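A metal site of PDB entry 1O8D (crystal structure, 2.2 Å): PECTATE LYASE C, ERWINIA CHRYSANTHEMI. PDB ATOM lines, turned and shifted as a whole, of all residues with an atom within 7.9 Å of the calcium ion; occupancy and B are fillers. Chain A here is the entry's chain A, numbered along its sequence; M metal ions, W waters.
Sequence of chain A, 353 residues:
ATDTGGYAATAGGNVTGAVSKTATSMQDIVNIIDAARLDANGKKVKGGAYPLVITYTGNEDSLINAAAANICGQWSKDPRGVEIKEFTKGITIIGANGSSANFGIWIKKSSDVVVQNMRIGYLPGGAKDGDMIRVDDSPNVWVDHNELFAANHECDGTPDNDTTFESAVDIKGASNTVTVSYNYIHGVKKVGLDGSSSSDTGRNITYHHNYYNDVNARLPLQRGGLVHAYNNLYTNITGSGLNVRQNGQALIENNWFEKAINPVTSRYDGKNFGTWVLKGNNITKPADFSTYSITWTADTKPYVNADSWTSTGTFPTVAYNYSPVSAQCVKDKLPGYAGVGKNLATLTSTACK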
ATOM      1  N   TRP A 106      22.037 -34.047 -13.251  1.00  0.00           N
ATOM      2  CA  TRP A 106      20.857 -33.213 -13.266  1.00  0.00           C
ATOM      3  C   TRP A 106      20.511 -32.763 -11.862  1.00  0.00           C
ATOM      4  O   TRP A 106      20.116 -33.564 -11.021  1.00  0.00           O
ATOM      5  CB  TRP A 106      19.710 -33.968 -13.928  1.00  0.00           C
ATOM      6  CG  TRP A 106      20.093 -34.529 -15.262  1.00  0.00           C
ATOM      7  CD1 TRP A 106      20.943 -33.974 -16.175  1.00  0.00           C
ATOM      8  CD2 TRP A 106      19.637 -35.756 -15.845  1.00  0.00           C
ATOM      9  NE1 TRP A 106      21.059 -34.774 -17.271  1.00  0.00           N
ATOM     10  CE2 TRP A 106      20.271 -35.876 -17.105  1.00  0.00           C
ATOM     11  CE3 TRP A 106      18.767 -36.768 -15.424  1.00  0.00           C
ATOM     12  CZ2 TRP A 106      20.061 -36.976 -17.952  1.00  0.00           C
ATOM     13  CZ3 TRP A 106      18.547 -37.864 -16.274  1.00  0.00           C
ATOM     14  CH2 TRP A 106      19.201 -37.957 -17.530  1.00  0.00           C
ATOM     15  N   GLY A 126      19.548 -37.211 -26.699  1.00  0.00           N
ATOM     16  CA  GLY A 126      19.327 -35.809 -27.024  1.00  0.00           C
ATOM     17  C   GLY A 126      17.859 -35.489 -27.221  1.00  0.00           C
ATOM     18  O   GLY A 126      17.419 -34.373 -26.925  1.00  0.00           O
ATOM     19  N   LYS A 128      15.477 -36.772 -25.587  1.00  0.00           N
ATOM     20  CA  LYS A 128      14.786 -36.868 -24.298  1.00  0.00           C
ATOM     21  C   LYS A 128      15.507 -36.150 -23.158  1.00  0.00           C
ATOM     22  O   LYS A 128      15.573 -36.659 -22.028  1.00  0.00           O
ATOM     23  CB  LYS A 128      14.504 -38.335 -23.943  1.00  0.00           C
ATOM     24  CG  LYS A 128      13.635 -39.053 -24.970  1.00  0.00           C
ATOM     25  CD  LYS A 128      13.353 -40.470 -24.526  1.00  0.00           C
ATOM     26  CE  LYS A 128      12.833 -41.304 -25.661  1.00  0.00           C
ATOM     27  NZ  LYS A 128      13.878 -41.525 -26.687  1.00  0.00           N
ATOM     28  N   ASP A 129      16.049 -34.963 -23.466  1.00  0.00           N
ATOM     29  CA  ASP A 129      16.732 -34.087 -22.512  1.00  0.00           C
ATOM     30  C   ASP A 129      17.999 -34.654 -21.878  1.00  0.00           C
ATOM     31  O   ASP A 129      18.199 -34.529 -20.672  1.00  0.00           O
ATOM     32  CB  ASP A 129      15.759 -33.620 -21.425  1.00  0.00           C
ATOM     33  CG  ASP A 129      15.837 -32.125 -21.156  1.00  0.00           C
ATOM     34  OD1 ASP A 129      16.535 -31.400 -21.889  1.00  0.00           O
ATOM     35  OD2 ASP A 129      15.191 -31.665 -20.191  1.00  0.00           O
ATOM     36  N   GLY A 130      18.882 -35.216 -22.695  1.00  0.00           N
ATOM     37  CA  GLY A 130      20.096 -35.775 -22.160  1.00  0.00           C
ATOM     38  C   GLY A 130      21.162 -34.724 -21.940  1.00  0.00           C
ATOM     39  O   GLY A 130      22.204 -34.794 -22.579  1.00  0.00           O
ATOM     40  N   ASP A 131      20.924 -33.784 -21.029  1.00  0.00           N
ATOM     41  CA  ASP A 131      21.884 -32.719 -20.736  1.00  0.00           C
ATOM     42  C   ASP A 131      23.102 -33.229 -19.991  1.00  0.00           C
ATOM     43  O   ASP A 131      23.009 -34.182 -19.221  1.00  0.00           O
ATOM     44  CB  ASP A 131      21.229 -31.637 -19.890  1.00  0.00           C
ATOM     45  CG  ASP A 131      20.135 -30.909 -20.631  1.00  0.00           C
ATOM     46  OD1 ASP A 131      20.317 -30.552 -21.808  1.00  0.00           O
ATOM     47  OD2 ASP A 131      19.085 -30.670 -20.014  1.00  0.00           O
ATOM     48  N   MET A 132      24.249 -32.585 -20.209  1.00  0.00           N
ATOM     49  CA  MET A 132      25.474 -32.960 -19.536  1.00  0.00           C
ATOM     50  C   MET A 132      25.339 -32.447 -18.128  1.00  0.00           C
ATOM     51  O   MET A 132      25.637 -33.136 -17.159  1.00  0.00           O
ATOM     52  CB  MET A 132      26.679 -32.349 -20.242  1.00  0.00           C
ATOM     53  CG  MET A 132      26.787 -32.793 -21.693  1.00  0.00           C
ATOM     54  SD  MET A 132      28.383 -32.478 -22.430  1.00  0.00           S
ATOM     55  CE  MET A 132      27.952 -31.568 -23.867  1.00  0.00           C
ATOM     56  N   ILE A 133      24.904 -31.203 -18.009  1.00  0.00           N
ATOM     57  CA  ILE A 133      24.659 -30.602 -16.709  1.00  0.00           C
ATOM     58  C   ILE A 133      23.398 -29.751 -16.832  1.00  0.00           C
ATOM     59  O   ILE A 133      23.178 -29.065 -17.839  1.00  0.00           O
ATOM     60  CB  ILE A 133      25.847 -29.770 -16.187  1.00  0.00           C
ATOM     61  CG1 ILE A 133      27.067 -30.672 -16.031  1.00  0.00           C
ATOM     62  CG2 ILE A 133      25.488 -29.138 -14.844  1.00  0.00           C
ATOM     63  CD1 ILE A 133      28.084 -30.159 -15.040  1.00  0.00           C
ATOM     64  N   ARG A 134      22.481 -29.945 -15.884  1.00  0.00           N
ATOM     65  CA  ARG A 134      21.242 -29.193 -15.846  1.00  0.00           C
ATOM     66  C   ARG A 134      21.079 -28.688 -14.428  1.00  0.00           C
ATOM     67  O   ARG A 134      21.286 -29.433 -13.487  1.00  0.00           O
ATOM     68  CB  ARG A 134      20.068 -30.089 -16.210  1.00  0.00           C
ATOM     69  CG  ARG A 134      18.756 -29.364 -16.185  1.00  0.00           C
ATOM     70  CD  ARG A 134      17.693 -30.093 -16.972  1.00  0.00           C
ATOM     71  NE  ARG A 134      17.302 -31.349 -16.349  1.00  0.00           N
ATOM     72  CZ  ARG A 134      17.358 -32.535 -16.950  1.00  0.00           C
ATOM     73  NH1 ARG A 134      17.801 -32.638 -18.187  1.00  0.00           N
ATOM     74  NH2 ARG A 134      16.882 -33.606 -16.337  1.00  0.00           N
ATOM     75  N   PHE A 165      22.069 -33.926 -29.929  1.00  0.00           N
ATOM     76  CA  PHE A 165      22.656 -33.875 -28.591  1.00  0.00           C
ATOM     77  C   PHE A 165      21.948 -32.753 -27.846  1.00  0.00           C
ATOM     78  O   PHE A 165      21.455 -31.801 -28.463  1.00  0.00           O
ATOM     79  CB  PHE A 165      24.164 -33.577 -28.633  1.00  0.00           C
ATOM     80  CG  PHE A 165      25.003 -34.742 -29.044  1.00  0.00           C
ATOM     81  CD1 PHE A 165      25.067 -35.889 -28.258  1.00  0.00           C
ATOM     82  CD2 PHE A 165      25.715 -34.721 -30.245  1.00  0.00           C
ATOM     83  CE1 PHE A 165      25.808 -37.003 -28.652  1.00  0.00           C
ATOM     84  CE2 PHE A 165      26.454 -35.830 -30.663  1.00  0.00           C
ATOM     85  CZ  PHE A 165      26.504 -36.979 -29.869  1.00  0.00           C
ATOM     86  N   GLU A 166      21.848 -32.890 -26.531  1.00  0.00           N
ATOM     87  CA  GLU A 166      21.233 -31.846 -25.750  1.00  0.00           C
ATOM     88  C   GLU A 166      22.330 -30.881 -25.308  1.00  0.00           C
ATOM     89  O   GLU A 166      23.400 -30.877 -25.883  1.00  0.00           O
ATOM     90  CB  GLU A 166      20.437 -32.384 -24.573  1.00  0.00           C
ATOM     91  CG  GLU A 166      18.967 -32.079 -24.711  1.00  0.00           C
ATOM     92  CD  GLU A 166      18.686 -30.594 -24.927  1.00  0.00           C
ATOM     93  OE1 GLU A 166      18.894 -29.769 -24.009  1.00  0.00           O
ATOM     94  OE2 GLU A 166      18.236 -30.252 -26.031  1.00  0.00           O
ATOM     95  N   SER A 167      22.100 -30.157 -24.225  1.00  0.00           N
ATOM     96  CA  SER A 167      23.043 -29.131 -23.823  1.00  0.00           C
ATOM     97  C   SER A 167      24.162 -29.436 -22.848  1.00  0.00           C
ATOM     98  O   SER A 167      24.190 -30.486 -22.215  1.00  0.00           O
ATOM     99  CB  SER A 167      22.249 -27.932 -23.341  1.00  0.00           C
ATOM    100  OG  SER A 167      21.158 -27.718 -24.232  1.00  0.00           O
ATOM    101  N   ALA A 168      25.109 -28.515 -22.753  1.00  0.00           N
ATOM    102  CA  ALA A 168      26.246 -28.671 -21.865  1.00  0.00           C
ATOM    103  C   ALA A 168      25.874 -28.252 -20.454  1.00  0.00           C
ATOM    104  O   ALA A 168      26.073 -29.015 -19.507  1.00  0.00           O
ATOM    105  CB  ALA A 168      27.444 -27.873 -22.372  1.00  0.00           C
ATOM    106  N   VAL A 169      25.336 -27.040 -20.298  1.00  0.00           N
ATOM    107  CA  VAL A 169      24.956 -26.540 -18.973  1.00  0.00           C
ATOM    108  C   VAL A 169      23.677 -25.706 -19.027  1.00  0.00           C
ATOM    109  O   VAL A 169      23.730 -24.482 -19.093  1.00  0.00           O
ATOM    110  CB  VAL A 169      26.083 -25.643 -18.325  1.00  0.00           C
ATOM    111  CG1 VAL A 169      25.747 -25.350 -16.859  1.00  0.00           C
ATOM    112  CG2 VAL A 169      27.434 -26.311 -18.408  1.00  0.00           C
ATOM    113  N   ASP A 170      22.517 -26.379 -19.007  1.00  0.00           N
ATOM    114  CA  ASP A 170      21.230 -25.695 -19.038  1.00  0.00           C
ATOM    115  C   ASP A 170      20.874 -25.221 -17.645  1.00  0.00           C
ATOM    116  O   ASP A 170      21.068 -25.952 -16.679  1.00  0.00           O
ATOM    117  CB  ASP A 170      20.140 -26.632 -19.567  1.00  0.00           C
ATOM    118  CG  ASP A 170      20.017 -26.590 -21.093  1.00  0.00           C
ATOM    119  OD1 ASP A 170      20.662 -25.759 -21.747  1.00  0.00           O
ATOM    120  OD2 ASP A 170      19.230 -27.388 -21.640  1.00  0.00           O
ATOM    121  N   ILE A 171      20.400 -23.993 -17.527  1.00  0.00           N
ATOM    122  CA  ILE A 171      20.018 -23.413 -16.244  1.00  0.00           C
ATOM    123  C   ILE A 171      18.608 -22.847 -16.372  1.00  0.00           C
ATOM    124  O   ILE A 171      18.323 -22.082 -17.292  1.00  0.00           O
ATOM    125  CB  ILE A 171      20.984 -22.278 -15.825  1.00  0.00           C
ATOM    126  CG1 ILE A 171      22.402 -22.828 -15.669  1.00  0.00           C
ATOM    127  CG2 ILE A 171      20.477 -21.600 -14.559  1.00  0.00           C
ATOM    128  CD1 ILE A 171      23.506 -21.779 -15.669  1.00  0.00           C
ATOM    129  N   LYS A 172      17.729 -23.205 -15.453  1.00  0.00           N
ATOM    130  CA  LYS A 172      16.365 -22.720 -15.510  1.00  0.00           C
ATOM    131  C   LYS A 172      15.723 -22.644 -14.137  1.00  0.00           C
ATOM    132  O   LYS A 172      16.312 -23.094 -13.140  1.00  0.00           O
ATOM    133  CB  LYS A 172      15.518 -23.610 -16.424  1.00  0.00           C
ATOM    134  CG  LYS A 172      15.593 -25.082 -16.142  1.00  0.00           C
ATOM    135  CD  LYS A 172      14.606 -25.803 -17.016  1.00  0.00           C
ATOM    136  CE  LYS A 172      14.761 -27.289 -16.964  1.00  0.00           C
ATOM    137  NZ  LYS A 172      13.578 -27.960 -17.589  1.00  0.00           N
ATOM    138  N   LYS A 190      24.242 -26.725 -28.721  1.00  0.00           N
ATOM    139  CA  LYS A 190      23.490 -25.836 -27.831  1.00  0.00           C
ATOM    140  C   LYS A 190      24.168 -25.859 -26.481  1.00  0.00           C
ATOM    141  O   LYS A 190      23.996 -26.786 -25.714  1.00  0.00           O
ATOM    142  CB  LYS A 190      22.049 -26.321 -27.695  1.00  0.00           C
ATOM    143  CG  LYS A 190      21.276 -26.278 -29.005  1.00  0.00           C
ATOM    144  CD  LYS A 190      20.635 -27.610 -29.311  1.00  0.00           C
ATOM    145  CE  LYS A 190      19.710 -28.018 -28.207  1.00  0.00           C
ATOM    146  NZ  LYS A 190      19.186 -29.378 -28.459  1.00  0.00           N
ATOM    147  N   GLY A 192      23.973 -23.802 -23.576  1.00  0.00           N
ATOM    148  CA  GLY A 192      23.163 -23.734 -22.383  1.00  0.00           C
ATOM    149  C   GLY A 192      22.176 -22.596 -22.336  1.00  0.00           C
ATOM    150  O   GLY A 192      22.452 -21.480 -22.765  1.00  0.00           O
ATOM    151  N   LEU A 193      20.992 -22.913 -21.804  1.00  0.00           N
ATOM    152  CA  LEU A 193      19.922 -21.950 -21.631  1.00  0.00           C
ATOM    153  C   LEU A 193      20.164 -21.213 -20.336  1.00  0.00           C
ATOM    154  O   LEU A 193      20.979 -21.624 -19.507  1.00  0.00           O
ATOM    155  CB  LEU A 193      18.565 -22.656 -21.492  1.00  0.00           C
ATOM    156  CG  LEU A 193      18.093 -23.492 -22.673  1.00  0.00           C
ATOM    157  CD1 LEU A 193      16.845 -24.271 -22.335  1.00  0.00           C
ATOM    158  CD2 LEU A 193      17.799 -22.582 -23.812  1.00  0.00           C
ATOM    159  N   ARG A 218      24.099 -20.267 -27.897  1.00  0.00           N
ATOM    160  CA  ARG A 218      23.646 -20.205 -26.506  1.00  0.00           C
ATOM    161  C   ARG A 218      24.794 -20.138 -25.505  1.00  0.00           C
ATOM    162  O   ARG A 218      25.020 -21.083 -24.745  1.00  0.00           O
ATOM    163  CB  ARG A 218      22.724 -21.381 -26.184  1.00  0.00           C
ATOM    164  CG  ARG A 218      21.657 -21.606 -27.208  1.00  0.00           C
ATOM    165  CD  ARG A 218      20.652 -22.574 -26.699  1.00  0.00           C
ATOM    166  NE  ARG A 218      19.586 -22.769 -27.657  1.00  0.00           N
ATOM    167  CZ  ARG A 218      18.622 -23.683 -27.519  1.00  0.00           C
ATOM    168  NH1 ARG A 218      18.603 -24.481 -26.458  1.00  0.00           N
ATOM    169  NH2 ARG A 218      17.690 -23.796 -28.452  1.00  0.00           N
HETATM  170 CA    CA M   1      18.122 -29.491 -21.771  1.00  0.00          CA
HETATM  171  O   HOH W   1      16.618 -28.639 -19.951  1.00  0.00           O
HETATM  172  O   HOH W   2      16.577 -28.209 -22.859  1.00  0.00           O
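N of Ser 167 lies close to OD1 of Asp 131. The guanidinium group (NH1) of Arg 134 lies close to the side-chain carboxylate (OD2) of Asp 131 (3.0 Å). O of Asp 131 sits at hydrogen-bond distance from NE1 of Trp 106 (2.8 Å). OD1 of Asp 170 lies close to OG of Ser 167. The side-chain carboxylate (OD1) of Asp 170 lies within hydrogen-bond range of the backbone NH (N) of Leu 193 (2.9 Å). The side-chain carboxylate (OE1) of Glu 166 lies close to the side-chain hydroxyl (OG) of Ser 167 (3.1 Å). OE2 of Glu 166 lies within salt-bridge range of NZ of Lys 190 (2.7 Å). The side-chain carboxylate (OD2) of Asp 129 lies within salt-bridge range of the guanidinium group (NH1) of Arg 134.
Of the 21 residues printed, 4 come within 4 Å of the calcium ion. Along chain A the residues within 4 Å of the calcium ion span positions 129 to 170. The nearest printed residue that does not touch the calcium ion is Ser 167 (4.3 Å).
The calcium ion is bound by water W2 (2.3 Å), OD2 of Asp 131 (2.3 Å), OD2 of Asp 170 (2.4 Å), OE1 of Glu 166 (2.4 Å), OD1 of Asp 131 (2.4 Å), OD1 of Asp 129 (2.5 Å) and water W1 (2.5 Å). The calcium ion has seven donor atoms within binding distance.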
